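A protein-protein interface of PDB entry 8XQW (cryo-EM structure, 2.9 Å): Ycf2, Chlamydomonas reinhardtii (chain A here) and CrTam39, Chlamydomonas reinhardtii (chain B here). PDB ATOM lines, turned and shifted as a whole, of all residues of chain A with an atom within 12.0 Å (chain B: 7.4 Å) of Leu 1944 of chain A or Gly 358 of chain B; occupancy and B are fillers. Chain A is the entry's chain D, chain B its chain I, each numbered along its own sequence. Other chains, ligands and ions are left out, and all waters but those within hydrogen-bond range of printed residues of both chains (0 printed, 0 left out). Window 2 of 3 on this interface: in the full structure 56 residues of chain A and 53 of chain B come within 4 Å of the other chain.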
ATOM      1  N   SER A 318      -0.156 -17.778  -8.731  1.00  0.00           N
ATOM      2  CA  SER A 318       0.823 -18.223  -7.749  1.00  0.00           C
ATOM      3  C   SER A 318       0.323 -18.073  -6.322  1.00  0.00           C
ATOM      4  O   SER A 318       1.074 -18.280  -5.380  1.00  0.00           O
ATOM      5  CB  SER A 318       2.126 -17.447  -7.902  1.00  0.00           C
ATOM      6  OG  SER A 318       2.739 -17.260  -6.639  1.00  0.00           O
ATOM      7  N   LEU A 319      -0.944 -17.714  -6.164  1.00  0.00           N
ATOM      8  CA  LEU A 319      -1.539 -17.520  -4.856  1.00  0.00           C
ATOM      9  C   LEU A 319      -2.140 -18.822  -4.341  1.00  0.00           C
ATOM     10  O   LEU A 319      -2.262 -19.811  -5.059  1.00  0.00           O
ATOM     11  CB  LEU A 319      -2.605 -16.434  -4.912  1.00  0.00           C
ATOM     12  CG  LEU A 319      -2.260 -15.155  -4.174  1.00  0.00           C
ATOM     13  CD1 LEU A 319      -1.282 -14.363  -4.985  1.00  0.00           C
ATOM     14  CD2 LEU A 319      -3.507 -14.360  -3.901  1.00  0.00           C
ATOM     15  N   TYR A 320      -2.520 -18.812  -3.072  1.00  0.00           N
ATOM     16  CA  TYR A 320      -3.250 -19.913  -2.475  1.00  0.00           C
ATOM     17  C   TYR A 320      -4.747 -19.662  -2.591  1.00  0.00           C
ATOM     18  O   TYR A 320      -5.193 -18.664  -3.151  1.00  0.00           O
ATOM     19  CB  TYR A 320      -2.853 -20.090  -1.015  1.00  0.00           C
ATOM     20  CG  TYR A 320      -1.491 -20.689  -0.806  1.00  0.00           C
ATOM     21  CD1 TYR A 320      -0.938 -21.540  -1.729  1.00  0.00           C
ATOM     22  CD2 TYR A 320      -0.765 -20.401   0.315  1.00  0.00           C
ATOM     23  CE1 TYR A 320       0.297 -22.081  -1.533  1.00  0.00           C
ATOM     24  CE2 TYR A 320       0.466 -20.937   0.515  1.00  0.00           C
ATOM     25  CZ  TYR A 320       0.991 -21.772  -0.411  1.00  0.00           C
ATOM     26  OH  TYR A 320       2.228 -22.311  -0.216  1.00  0.00           O
ATOM     27  N   PHE A 321      -5.531 -20.586  -2.047  1.00  0.00           N
ATOM     28  CA  PHE A 321      -6.989 -20.496  -2.078  1.00  0.00           C
ATOM     29  C   PHE A 321      -7.473 -20.069  -0.698  1.00  0.00           C
ATOM     30  O   PHE A 321      -7.888 -20.877   0.130  1.00  0.00           O
ATOM     31  CB  PHE A 321      -7.584 -21.832  -2.490  1.00  0.00           C
ATOM     32  CG  PHE A 321      -8.966 -21.741  -3.052  1.00  0.00           C
ATOM     33  CD1 PHE A 321      -9.239 -20.928  -4.129  1.00  0.00           C
ATOM     34  CD2 PHE A 321      -9.985 -22.501  -2.520  1.00  0.00           C
ATOM     35  CE1 PHE A 321     -10.506 -20.865  -4.647  1.00  0.00           C
ATOM     36  CE2 PHE A 321     -11.248 -22.437  -3.038  1.00  0.00           C
ATOM     37  CZ  PHE A 321     -11.508 -21.620  -4.102  1.00  0.00           C
ATOM     38  N   VAL A 322      -7.420 -18.766  -0.449  1.00  0.00           N
ATOM     39  CA  VAL A 322      -7.723 -18.224   0.867  1.00  0.00           C
ATOM     40  C   VAL A 322      -8.523 -16.938   0.712  1.00  0.00           C
ATOM     41  O   VAL A 322      -8.413 -16.232  -0.292  1.00  0.00           O
ATOM     42  CB  VAL A 322      -6.438 -17.975   1.685  1.00  0.00           C
ATOM     43  CG1 VAL A 322      -5.798 -19.278   2.062  1.00  0.00           C
ATOM     44  CG2 VAL A 322      -5.465 -17.147   0.901  1.00  0.00           C
ATOM     45  N   PHE A 323      -9.341 -16.646   1.717  1.00  0.00           N
ATOM     46  CA  PHE A 323     -10.110 -15.415   1.737  1.00  0.00           C
ATOM     47  C   PHE A 323      -9.190 -14.217   1.911  1.00  0.00           C
ATOM     48  O   PHE A 323      -7.998 -14.351   2.179  1.00  0.00           O
ATOM     49  CB  PHE A 323     -11.114 -15.424   2.878  1.00  0.00           C
ATOM     50  CG  PHE A 323     -12.262 -16.358   2.690  1.00  0.00           C
ATOM     51  CD1 PHE A 323     -13.356 -15.985   1.950  1.00  0.00           C
ATOM     52  CD2 PHE A 323     -12.268 -17.588   3.297  1.00  0.00           C
ATOM     53  CE1 PHE A 323     -14.413 -16.825   1.803  1.00  0.00           C
ATOM     54  CE2 PHE A 323     -13.323 -18.436   3.141  1.00  0.00           C
ATOM     55  CZ  PHE A 323     -14.397 -18.051   2.399  1.00  0.00           C
ATOM     56  N   THR A 324      -9.762 -13.030   1.777  1.00  0.00           N
ATOM     57  CA  THR A 324      -9.052 -11.799   2.078  1.00  0.00           C
ATOM     58  C   THR A 324      -9.621 -11.191   3.358  1.00  0.00           C
ATOM     59  O   THR A 324     -10.651 -11.627   3.869  1.00  0.00           O
ATOM     60  CB  THR A 324      -9.122 -10.840   0.899  1.00  0.00           C
ATOM     61  OG1 THR A 324     -10.313 -11.098   0.152  1.00  0.00           O
ATOM     62  CG2 THR A 324      -7.925 -11.007   0.010  1.00  0.00           C
ATOM     63  N   GLN A 325      -8.967 -10.161   3.880  1.00  0.00           N
ATOM     64  CA  GLN A 325      -9.181  -9.791   5.271  1.00  0.00           C
ATOM     65  C   GLN A 325     -10.573  -9.240   5.546  1.00  0.00           C
ATOM     66  O   GLN A 325     -11.181  -9.608   6.555  1.00  0.00           O
ATOM     67  CB  GLN A 325      -8.134  -8.777   5.715  1.00  0.00           C
ATOM     68  CG  GLN A 325      -7.882  -8.823   7.193  1.00  0.00           C
ATOM     69  CD  GLN A 325      -7.307  -7.543   7.713  1.00  0.00           C
ATOM     70  OE1 GLN A 325      -7.496  -7.190   8.871  1.00  0.00           O
ATOM     71  NE2 GLN A 325      -6.596  -6.832   6.857  1.00  0.00           N
ATOM     72  N   LEU A 326     -11.063  -8.335   4.700  1.00  0.00           N
ATOM     73  CA  LEU A 326     -12.452  -7.875   4.721  1.00  0.00           C
ATOM     74  C   LEU A 326     -12.777  -6.900   5.848  1.00  0.00           C
ATOM     75  O   LEU A 326     -13.876  -6.348   5.878  1.00  0.00           O
ATOM     76  CB  LEU A 326     -13.398  -9.075   4.797  1.00  0.00           C
ATOM     77  CG  LEU A 326     -14.893  -8.897   4.605  1.00  0.00           C
ATOM     78  CD1 LEU A 326     -15.252  -9.416   3.253  1.00  0.00           C
ATOM     79  CD2 LEU A 326     -15.630  -9.652   5.667  1.00  0.00           C
ATOM     80  N   ASN A 327     -11.851  -6.642   6.766  1.00  0.00           N
ATOM     81  CA  ASN A 327     -12.149  -5.627   7.769  1.00  0.00           C
ATOM     82  C   ASN A 327     -11.024  -4.617   7.942  1.00  0.00           C
ATOM     83  O   ASN A 327     -10.972  -3.936   8.971  1.00  0.00           O
ATOM     84  CB  ASN A 327     -12.493  -6.257   9.125  1.00  0.00           C
ATOM     85  CG  ASN A 327     -11.338  -7.017   9.747  1.00  0.00           C
ATOM     86  OD1 ASN A 327     -10.175  -6.668   9.585  1.00  0.00           O
ATOM     87  ND2 ASN A 327     -11.669  -8.061  10.492  1.00  0.00           N
ATOM     88  N   GLN A 328     -10.121  -4.500   6.975  1.00  0.00           N
ATOM     89  CA  GLN A 328      -9.064  -3.506   7.073  1.00  0.00           C
ATOM     90  C   GLN A 328      -9.555  -2.115   6.730  1.00  0.00           C
ATOM     91  O   GLN A 328      -8.898  -1.133   7.082  1.00  0.00           O
ATOM     92  CB  GLN A 328      -7.903  -3.883   6.154  1.00  0.00           C
ATOM     93  CG  GLN A 328      -6.613  -3.127   6.425  1.00  0.00           C
ATOM     94  CD  GLN A 328      -6.221  -3.132   7.888  1.00  0.00           C
ATOM     95  OE1 GLN A 328      -6.303  -4.155   8.562  1.00  0.00           O
ATOM     96  NE2 GLN A 328      -5.793  -1.983   8.386  1.00  0.00           N
ATOM     97  N   LYS A 329     -10.700  -2.010   6.069  1.00  0.00           N
ATOM     98  CA  LYS A 329     -11.246  -0.729   5.651  1.00  0.00           C
ATOM     99  C   LYS A 329     -12.245  -0.169   6.652  1.00  0.00           C
ATOM    100  O   LYS A 329     -12.063   0.938   7.155  1.00  0.00           O
ATOM    101  CB  LYS A 329     -11.906  -0.884   4.284  1.00  0.00           C
ATOM    102  CG  LYS A 329     -11.746   0.292   3.371  1.00  0.00           C
ATOM    103  CD  LYS A 329     -11.658  -0.171   1.940  1.00  0.00           C
ATOM    104  CE  LYS A 329     -12.040   0.930   0.978  1.00  0.00           C
ATOM    105  NZ  LYS A 329     -11.214   2.149   1.172  1.00  0.00           N
ATOM    106  N   THR A 330     -13.292  -0.927   6.968  1.00  0.00           N
ATOM    107  CA  THR A 330     -14.379  -0.424   7.796  1.00  0.00           C
ATOM    108  C   THR A 330     -14.650  -1.342   8.977  1.00  0.00           C
ATOM    109  O   THR A 330     -13.858  -2.235   9.278  1.00  0.00           O
ATOM    110  CB  THR A 330     -15.661  -0.282   6.980  1.00  0.00           C
ATOM    111  OG1 THR A 330     -16.287  -1.560   6.866  1.00  0.00           O
ATOM    112  CG2 THR A 330     -15.361   0.221   5.591  1.00  0.00           C
ATOM    113  N   TYR A1920     -12.539  -1.554 -10.918  1.00  0.00           N
ATOM    114  CA  TYR A1920     -12.428  -2.995 -10.734  1.00  0.00           C
ATOM    115  C   TYR A1920     -13.164  -3.777 -11.810  1.00  0.00           C
ATOM    116  O   TYR A1920     -12.908  -4.972 -11.967  1.00  0.00           O
ATOM    117  CB  TYR A1920     -12.952  -3.400  -9.361  1.00  0.00           C
ATOM    118  CG  TYR A1920     -12.250  -2.733  -8.210  1.00  0.00           C
ATOM    119  CD1 TYR A1920     -11.114  -3.287  -7.648  1.00  0.00           C
ATOM    120  CD2 TYR A1920     -12.732  -1.552  -7.676  1.00  0.00           C
ATOM    121  CE1 TYR A1920     -10.478  -2.679  -6.593  1.00  0.00           C
ATOM    122  CE2 TYR A1920     -12.103  -0.940  -6.622  1.00  0.00           C
ATOM    123  CZ  TYR A1920     -10.980  -1.507  -6.084  1.00  0.00           C
ATOM    124  OH  TYR A1920     -10.352  -0.889  -5.030  1.00  0.00           O
ATOM    125  N   LEU A1944      -2.660  -2.746   3.366  1.00  0.00           N
ATOM    126  CA  LEU A1944      -2.570  -4.198   3.453  1.00  0.00           C
ATOM    127  C   LEU A1944      -2.284  -4.661   4.877  1.00  0.00           C
ATOM    128  O   LEU A1944      -2.112  -5.853   5.124  1.00  0.00           O
ATOM    129  CB  LEU A1944      -1.494  -4.723   2.499  1.00  0.00           C
ATOM    130  CG  LEU A1944      -1.582  -6.188   2.059  1.00  0.00           C
ATOM    131  CD1 LEU A1944      -3.006  -6.715   2.150  1.00  0.00           C
ATOM    132  CD2 LEU A1944      -1.048  -6.351   0.649  1.00  0.00           C
ATOM    133  N   ASN A1945      -2.260  -3.716   5.818  1.00  0.00           N
ATOM    134  CA  ASN A1945      -1.970  -4.018   7.215  1.00  0.00           C
ATOM    135  C   ASN A1945      -0.597  -4.680   7.345  1.00  0.00           C
ATOM    136  O   ASN A1945      -0.461  -5.876   7.589  1.00  0.00           O
ATOM    137  CB  ASN A1945      -3.058  -4.891   7.844  1.00  0.00           C
ATOM    138  CG  ASN A1945      -3.008  -4.868   9.352  1.00  0.00           C
ATOM    139  OD1 ASN A1945      -2.404  -3.980   9.947  1.00  0.00           O
ATOM    140  ND2 ASN A1945      -3.643  -5.847   9.981  1.00  0.00           N
ATOM    141  N   ARG A1946       0.416  -3.862   7.097  1.00  0.00           N
ATOM    142  CA  ARG A1946       1.807  -4.247   7.274  1.00  0.00           C
ATOM    143  C   ARG A1946       2.060  -4.982   8.585  1.00  0.00           C
ATOM    144  O   ARG A1946       2.951  -5.827   8.657  1.00  0.00           O
ATOM    145  CB  ARG A1946       2.671  -2.995   7.182  1.00  0.00           C
ATOM    146  CG  ARG A1946       4.014  -3.097   7.836  1.00  0.00           C
ATOM    147  CD  ARG A1946       4.581  -1.724   8.098  1.00  0.00           C
ATOM    148  NE  ARG A1946       5.912  -1.804   8.685  1.00  0.00           N
ATOM    149  CZ  ARG A1946       6.146  -2.091   9.958  1.00  0.00           C
ATOM    150  NH1 ARG A1946       7.387  -2.145  10.408  1.00  0.00           N
ATOM    151  NH2 ARG A1946       5.135  -2.320  10.781  1.00  0.00           N
ATOM    152  N   TRP A1947       1.280  -4.692   9.623  1.00  0.00           N
ATOM    153  CA  TRP A1947       1.491  -5.327  10.916  1.00  0.00           C
ATOM    154  C   TRP A1947       1.127  -6.803  10.927  1.00  0.00           C
ATOM    155  O   TRP A1947       1.273  -7.451  11.964  1.00  0.00           O
ATOM    156  CB  TRP A1947       0.684  -4.600  11.986  1.00  0.00           C
ATOM    157  CG  TRP A1947       1.043  -4.985  13.374  1.00  0.00           C
ATOM    158  CD1 TRP A1947       0.335  -5.791  14.202  1.00  0.00           C
ATOM    159  CD2 TRP A1947       2.202  -4.586  14.100  1.00  0.00           C
ATOM    160  NE1 TRP A1947       0.978  -5.920  15.400  1.00  0.00           N
ATOM    161  CE2 TRP A1947       2.130  -5.186  15.361  1.00  0.00           C
ATOM    162  CE3 TRP A1947       3.293  -3.772  13.807  1.00  0.00           C
ATOM    163  CZ2 TRP A1947       3.096  -5.006  16.320  1.00  0.00           C
ATOM    164  CZ3 TRP A1947       4.250  -3.594  14.758  1.00  0.00           C
ATOM    165  CH2 TRP A1947       4.150  -4.205  16.002  1.00  0.00           C
ATOM    166  N   SER A1948       0.658  -7.354   9.822  1.00  0.00           N
ATOM    167  CA  SER A1948       0.295  -8.759   9.815  1.00  0.00           C
ATOM    168  C   SER A1948       1.464  -9.670   9.513  1.00  0.00           C
ATOM    169  O   SER A1948       1.414 -10.847   9.866  1.00  0.00           O
ATOM    170  CB  SER A1948      -0.804  -9.020   8.793  1.00  0.00           C
ATOM    171  OG  SER A1948      -1.904  -8.171   9.022  1.00  0.00           O
ATOM    172  N   VAL A1949       2.510  -9.166   8.866  1.00  0.00           N
ATOM    173  CA  VAL A1949       3.611 -10.011   8.434  1.00  0.00           C
ATOM    174  C   VAL A1949       4.948  -9.404   8.816  1.00  0.00           C
ATOM    175  O   VAL A1949       5.995 -10.020   8.613  1.00  0.00           O
ATOM    176  CB  VAL A1949       3.548 -10.248   6.922  1.00  0.00           C
ATOM    177  CG1 VAL A1949       2.428 -11.163   6.607  1.00  0.00           C
ATOM    178  CG2 VAL A1949       3.359  -8.957   6.217  1.00  0.00           C
ATOM    179  N   ASN A1950       4.931  -8.194   9.355  1.00  0.00           N
ATOM    180  CA  ASN A1950       6.157  -7.459   9.636  1.00  0.00           C
ATOM    181  C   ASN A1950       5.928  -6.615  10.874  1.00  0.00           C
ATOM    182  O   ASN A1950       5.363  -5.526  10.784  1.00  0.00           O
ATOM    183  CB  ASN A1950       6.541  -6.584   8.452  1.00  0.00           C
ATOM    184  CG  ASN A1950       7.880  -5.946   8.614  1.00  0.00           C
ATOM    185  OD1 ASN A1950       8.503  -6.037   9.660  1.00  0.00           O
ATOM    186  ND2 ASN A1950       8.343  -5.291   7.570  1.00  0.00           N
ATOM    187  N   GLN A1951       6.375  -7.105  12.025  1.00  0.00           N
ATOM    188  CA  GLN A1951       6.208  -6.403  13.286  1.00  0.00           C
ATOM    189  C   GLN A1951       7.496  -5.750  13.760  1.00  0.00           C
ATOM    190  O   GLN A1951       7.764  -5.722  14.958  1.00  0.00           O
ATOM    191  CB  GLN A1951       5.680  -7.359  14.348  1.00  0.00           C
ATOM    192  CG  GLN A1951       5.749  -8.791  13.939  1.00  0.00           C
ATOM    193  CD  GLN A1951       4.458  -9.289  13.402  1.00  0.00           C
ATOM    194  OE1 GLN A1951       4.420 -10.185  12.573  1.00  0.00           O
ATOM    195  NE2 GLN A1951       3.379  -8.723  13.883  1.00  0.00           N
ATOM    196  N   PRO B 338       3.787 -16.751   6.810  1.00  0.00           N
ATOM    197  CA  PRO B 338       4.605 -15.564   7.030  1.00  0.00           C
ATOM    198  C   PRO B 338       5.068 -15.415   8.455  1.00  0.00           C
ATOM    199  O   PRO B 338       5.763 -14.444   8.759  1.00  0.00           O
ATOM    200  CB  PRO B 338       3.667 -14.426   6.652  1.00  0.00           C
ATOM    201  CG  PRO B 338       2.731 -15.009   5.760  1.00  0.00           C
ATOM    202  CD  PRO B 338       2.516 -16.401   6.181  1.00  0.00           C
ATOM    203  N   SER B 352       9.227 -14.912  -1.331  1.00  0.00           N
ATOM    204  CA  SER B 352       8.416 -15.939  -1.974  1.00  0.00           C
ATOM    205  C   SER B 352       7.211 -16.311  -1.123  1.00  0.00           C
ATOM    206  O   SER B 352       6.084 -16.419  -1.625  1.00  0.00           O
ATOM    207  CB  SER B 352       9.275 -17.165  -2.244  1.00  0.00           C
ATOM    208  OG  SER B 352       8.510 -18.338  -2.124  1.00  0.00           O
ATOM    209  N   VAL B 353       7.427 -16.508   0.174  1.00  0.00           N
ATOM    210  CA  VAL B 353       6.332 -16.924   1.049  1.00  0.00           C
ATOM    211  C   VAL B 353       5.292 -15.818   1.173  1.00  0.00           C
ATOM    212  O   VAL B 353       4.084 -16.065   1.073  1.00  0.00           O
ATOM    213  CB  VAL B 353       6.876 -17.343   2.422  1.00  0.00           C
ATOM    214  CG1 VAL B 353       5.780 -17.387   3.407  1.00  0.00           C
ATOM    215  CG2 VAL B 353       7.492 -18.684   2.324  1.00  0.00           C
ATOM    216  N   TRP B 354       5.740 -14.585   1.398  1.00  0.00           N
ATOM    217  CA  TRP B 354       4.810 -13.467   1.457  1.00  0.00           C
ATOM    218  C   TRP B 354       3.989 -13.374   0.187  1.00  0.00           C
ATOM    219  O   TRP B 354       2.789 -13.111   0.232  1.00  0.00           O
ATOM    220  CB  TRP B 354       5.556 -12.166   1.671  1.00  0.00           C
ATOM    221  CG  TRP B 354       6.081 -11.965   3.008  1.00  0.00           C
ATOM    222  CD1 TRP B 354       6.228 -12.889   3.974  1.00  0.00           C
ATOM    223  CD2 TRP B 354       6.565 -10.743   3.536  1.00  0.00           C
ATOM    224  NE1 TRP B 354       6.773 -12.322   5.091  1.00  0.00           N
ATOM    225  CE2 TRP B 354       6.983 -10.995   4.844  1.00  0.00           C
ATOM    226  CE3 TRP B 354       6.672  -9.452   3.035  1.00  0.00           C
ATOM    227  CZ2 TRP B 354       7.513 -10.007   5.653  1.00  0.00           C
ATOM    228  CZ3 TRP B 354       7.192  -8.480   3.839  1.00  0.00           C
ATOM    229  CH2 TRP B 354       7.602  -8.756   5.128  1.00  0.00           C
ATOM    230  N   GLN B 355       4.628 -13.559  -0.962  1.00  0.00           N
ATOM    231  CA  GLN B 355       3.907 -13.514  -2.225  1.00  0.00           C
ATOM    232  C   GLN B 355       2.806 -14.551  -2.266  1.00  0.00           C
ATOM    233  O   GLN B 355       1.672 -14.253  -2.646  1.00  0.00           O
ATOM    234  CB  GLN B 355       4.877 -13.733  -3.376  1.00  0.00           C
ATOM    235  CG  GLN B 355       4.216 -14.127  -4.663  1.00  0.00           C
ATOM    236  CD  GLN B 355       3.535 -12.973  -5.339  1.00  0.00           C
ATOM    237  OE1 GLN B 355       2.586 -13.158  -6.097  1.00  0.00           O
ATOM    238  NE2 GLN B 355       4.015 -11.767  -5.074  1.00  0.00           N
ATOM    239  N   LYS B 356       3.123 -15.786  -1.884  1.00  0.00           N
ATOM    240  CA  LYS B 356       2.123 -16.844  -1.961  1.00  0.00           C
ATOM    241  C   LYS B 356       0.953 -16.591  -1.034  1.00  0.00           C
ATOM    242  O   LYS B 356      -0.182 -16.933  -1.367  1.00  0.00           O
ATOM    243  CB  LYS B 356       2.753 -18.182  -1.635  1.00  0.00           C
ATOM    244  CG  LYS B 356       3.378 -18.837  -2.809  1.00  0.00           C
ATOM    245  CD  LYS B 356       4.279 -19.944  -2.355  1.00  0.00           C
ATOM    246  CE  LYS B 356       4.891 -20.654  -3.526  1.00  0.00           C
ATOM    247  NZ  LYS B 356       5.652 -21.841  -3.084  1.00  0.00           N
ATOM    248  N   TRP B 357       1.194 -16.018   0.132  1.00  0.00           N
ATOM    249  CA  TRP B 357       0.109 -15.847   1.086  1.00  0.00           C
ATOM    250  C   TRP B 357      -0.702 -14.583   0.861  1.00  0.00           C
ATOM    251  O   TRP B 357      -1.678 -14.366   1.573  1.00  0.00           O
ATOM    252  CB  TRP B 357       0.653 -15.872   2.509  1.00  0.00           C
ATOM    253  CG  TRP B 357       0.833 -17.245   2.995  1.00  0.00           C
ATOM    254  CD1 TRP B 357       1.951 -17.995   2.907  1.00  0.00           C
ATOM    255  CD2 TRP B 357      -0.148 -18.060   3.614  1.00  0.00           C
ATOM    256  NE1 TRP B 357       1.737 -19.226   3.443  1.00  0.00           N
ATOM    257  CE2 TRP B 357       0.447 -19.290   3.888  1.00  0.00           C
ATOM    258  CE3 TRP B 357      -1.476 -17.868   3.971  1.00  0.00           C
ATOM    259  CZ2 TRP B 357      -0.233 -20.317   4.498  1.00  0.00           C
ATOM    260  CZ3 TRP B 357      -2.142 -18.884   4.578  1.00  0.00           C
ATOM    261  CH2 TRP B 357      -1.526 -20.094   4.835  1.00  0.00           C
ATOM    262  N   GLY B 358      -0.343 -13.754  -0.101  1.00  0.00           N
ATOM    263  CA  GLY B 358      -1.133 -12.594  -0.430  1.00  0.00           C
ATOM    264  C   GLY B 358      -0.592 -11.267   0.032  1.00  0.00           C
ATOM    265  O   GLY B 358      -1.325 -10.281  -0.003  1.00  0.00           O
ATOM    266  N   TYR B 359       0.663 -11.204   0.464  1.00  0.00           N
ATOM    267  CA  TYR B 359       1.263  -9.977   0.964  1.00  0.00           C
ATOM    268  C   TYR B 359       2.395  -9.491   0.074  1.00  0.00           C
ATOM    269  O   TYR B 359       3.368  -8.926   0.565  1.00  0.00           O
ATOM    270  CB  TYR B 359       1.786 -10.170   2.378  1.00  0.00           C
ATOM    271  CG  TYR B 359       0.741 -10.592   3.353  1.00  0.00           C
ATOM    272  CD1 TYR B 359      -0.096  -9.669   3.931  1.00  0.00           C
ATOM    273  CD2 TYR B 359       0.586 -11.915   3.694  1.00  0.00           C
ATOM    274  CE1 TYR B 359      -1.047 -10.049   4.811  1.00  0.00           C
ATOM    275  CE2 TYR B 359      -0.371 -12.300   4.571  1.00  0.00           C
ATOM    276  CZ  TYR B 359      -1.182 -11.364   5.124  1.00  0.00           C
ATOM    277  OH  TYR B 359      -2.141 -11.747   6.014  1.00  0.00           O
ATOM    278  N   GLY B 360       2.281  -9.696  -1.233  1.00  0.00           N
ATOM    279  CA  GLY B 360       3.364  -9.351  -2.129  1.00  0.00           C
ATOM    280  C   GLY B 360       3.688  -7.876  -2.190  1.00  0.00           C
ATOM    281  O   GLY B 360       4.779  -7.515  -2.631  1.00  0.00           O
ATOM    282  N   GLN B 361       2.772  -7.019  -1.763  1.00  0.00           N
ATOM    283  CA  GLN B 361       2.961  -5.583  -1.884  1.00  0.00           C
ATOM    284  C   GLN B 361       3.462  -4.934  -0.608  1.00  0.00           C
ATOM    285  O   GLN B 361       3.810  -3.753  -0.633  1.00  0.00           O
ATOM    286  CB  GLN B 361       1.653  -4.921  -2.296  1.00  0.00           C
ATOM    287  CG  GLN B 361       0.974  -5.603  -3.453  1.00  0.00           C
ATOM    288  CD  GLN B 361       1.640  -5.298  -4.768  1.00  0.00           C
ATOM    289  OE1 GLN B 361       1.920  -4.143  -5.078  1.00  0.00           O
ATOM    290  NE2 GLN B 361       1.904  -6.332  -5.552  1.00  0.00           N
ATOM    291  N   VAL B 362       3.503  -5.662   0.502  1.00  0.00           N
ATOM    292  CA  VAL B 362       3.979  -5.087   1.746  1.00  0.00           C
ATOM    293  C   VAL B 362       5.455  -4.742   1.614  1.00  0.00           C
ATOM    294  O   VAL B 362       6.199  -5.359   0.845  1.00  0.00           O
ATOM    295  CB  VAL B 362       3.717  -6.060   2.906  1.00  0.00           C
ATOM    296  CG1 VAL B 362       4.024  -5.426   4.223  1.00  0.00           C
ATOM    297  CG2 VAL B 362       2.285  -6.483   2.886  1.00  0.00           C
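The backbone NH (N) of Tyr 320 of chain A lies within hydrogen-bond range of the backbone carbonyl oxygen (O) of Lys 356 of chain B, 3.5 Å away.
NH2 of Arg 1946 of chain A lies within hydrogen-bond range of O of Asn 1950 of chain A (3.2 Å).
The backbone carbonyl oxygen (O) of Trp 354 of chain B sits at hydrogen-bond distance from the backbone NH (N) of Tyr 359 of chain B (2.9 Å).
OG of Ser 318 of chain A touches CG of Gln 355 of chain B (3.99 Å).
Ser 318 of chain A touches Lys 356 of chain B (O to CG, 3.5 Å).
Leu 319 of chain A touches Gln 355 of chain B (CD1 to O, 3.8 Å).
Lys 356 of chain B touches Leu 319 of chain A (O to CA, 3.8 Å).
NE1 of Trp 357 of chain B touches CE2 of Tyr 320 of chain A, 3.6 Å away.
Gly 358 of chain B touches Leu 1944 of chain A.
CG of Leu 1944 of chain A touches CG2 of Val 362 of chain B (3.97 Å).
Val 1949 of chain A touches Pro 338 of chain B.
Trp 354 of chain B touches Val 1949 of chain A.
Val 1949 of chain A touches Tyr 359 of chain B (CG1 to CD2, 3.5 Å).
Of the printed residues of chain B, Leu 1944 of chain A touches Gly 358 (3.99 Å) and Val 362 (3.97 Å).
Of the printed residues of chain A, Gly 358 of chain B touches Leu 1944.
No residue of chain A comes within 4 Å of Gln 361 of chain B.
Of the printed residues of chain A, Val 362 of chain B touches Leu 1944 (3.97 Å) and Arg 1946 (3.95 Å).
Of the printed residues of chain B, Leu 319 of chain A touches Gln 355 and Lys 356.
Of the printed residues of chain B, Arg 1946 of chain A touches Val 362 (3.95 Å).
The nearest printed residue of chain B that does not touch Leu 1944 of chain A is Tyr 359 of chain B (4.2 Å).
The nearest printed residue of chain A that does not touch Trp 354 of chain B is Asn 1950 of chain A (4.1 Å).
Printed residues of chain B that touch a printed residue of chain A: Pro 338, Trp 354, Gln 355, Lys 356, Trp 357, Gly 358, Tyr 359 and Val 362.
Along chain B the printed residues that touch a printed residue of chain A span positions 338 to 362.
Of the 22 printed residues of chain A, 6 touch a printed residue of chain B.
Hydrophobic or aromatic side chains of chain A within 4 Å of the printed part of chain B: Leu 319, Tyr 320, Leu 1944 and Val 1949.
Among the printed residues, 12 pairs touch across the chains.
Among the printed residues, no Asp or Glu carboxylate lies within 4 Å of a Lys or Arg side-chain nitrogen of the other chain.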
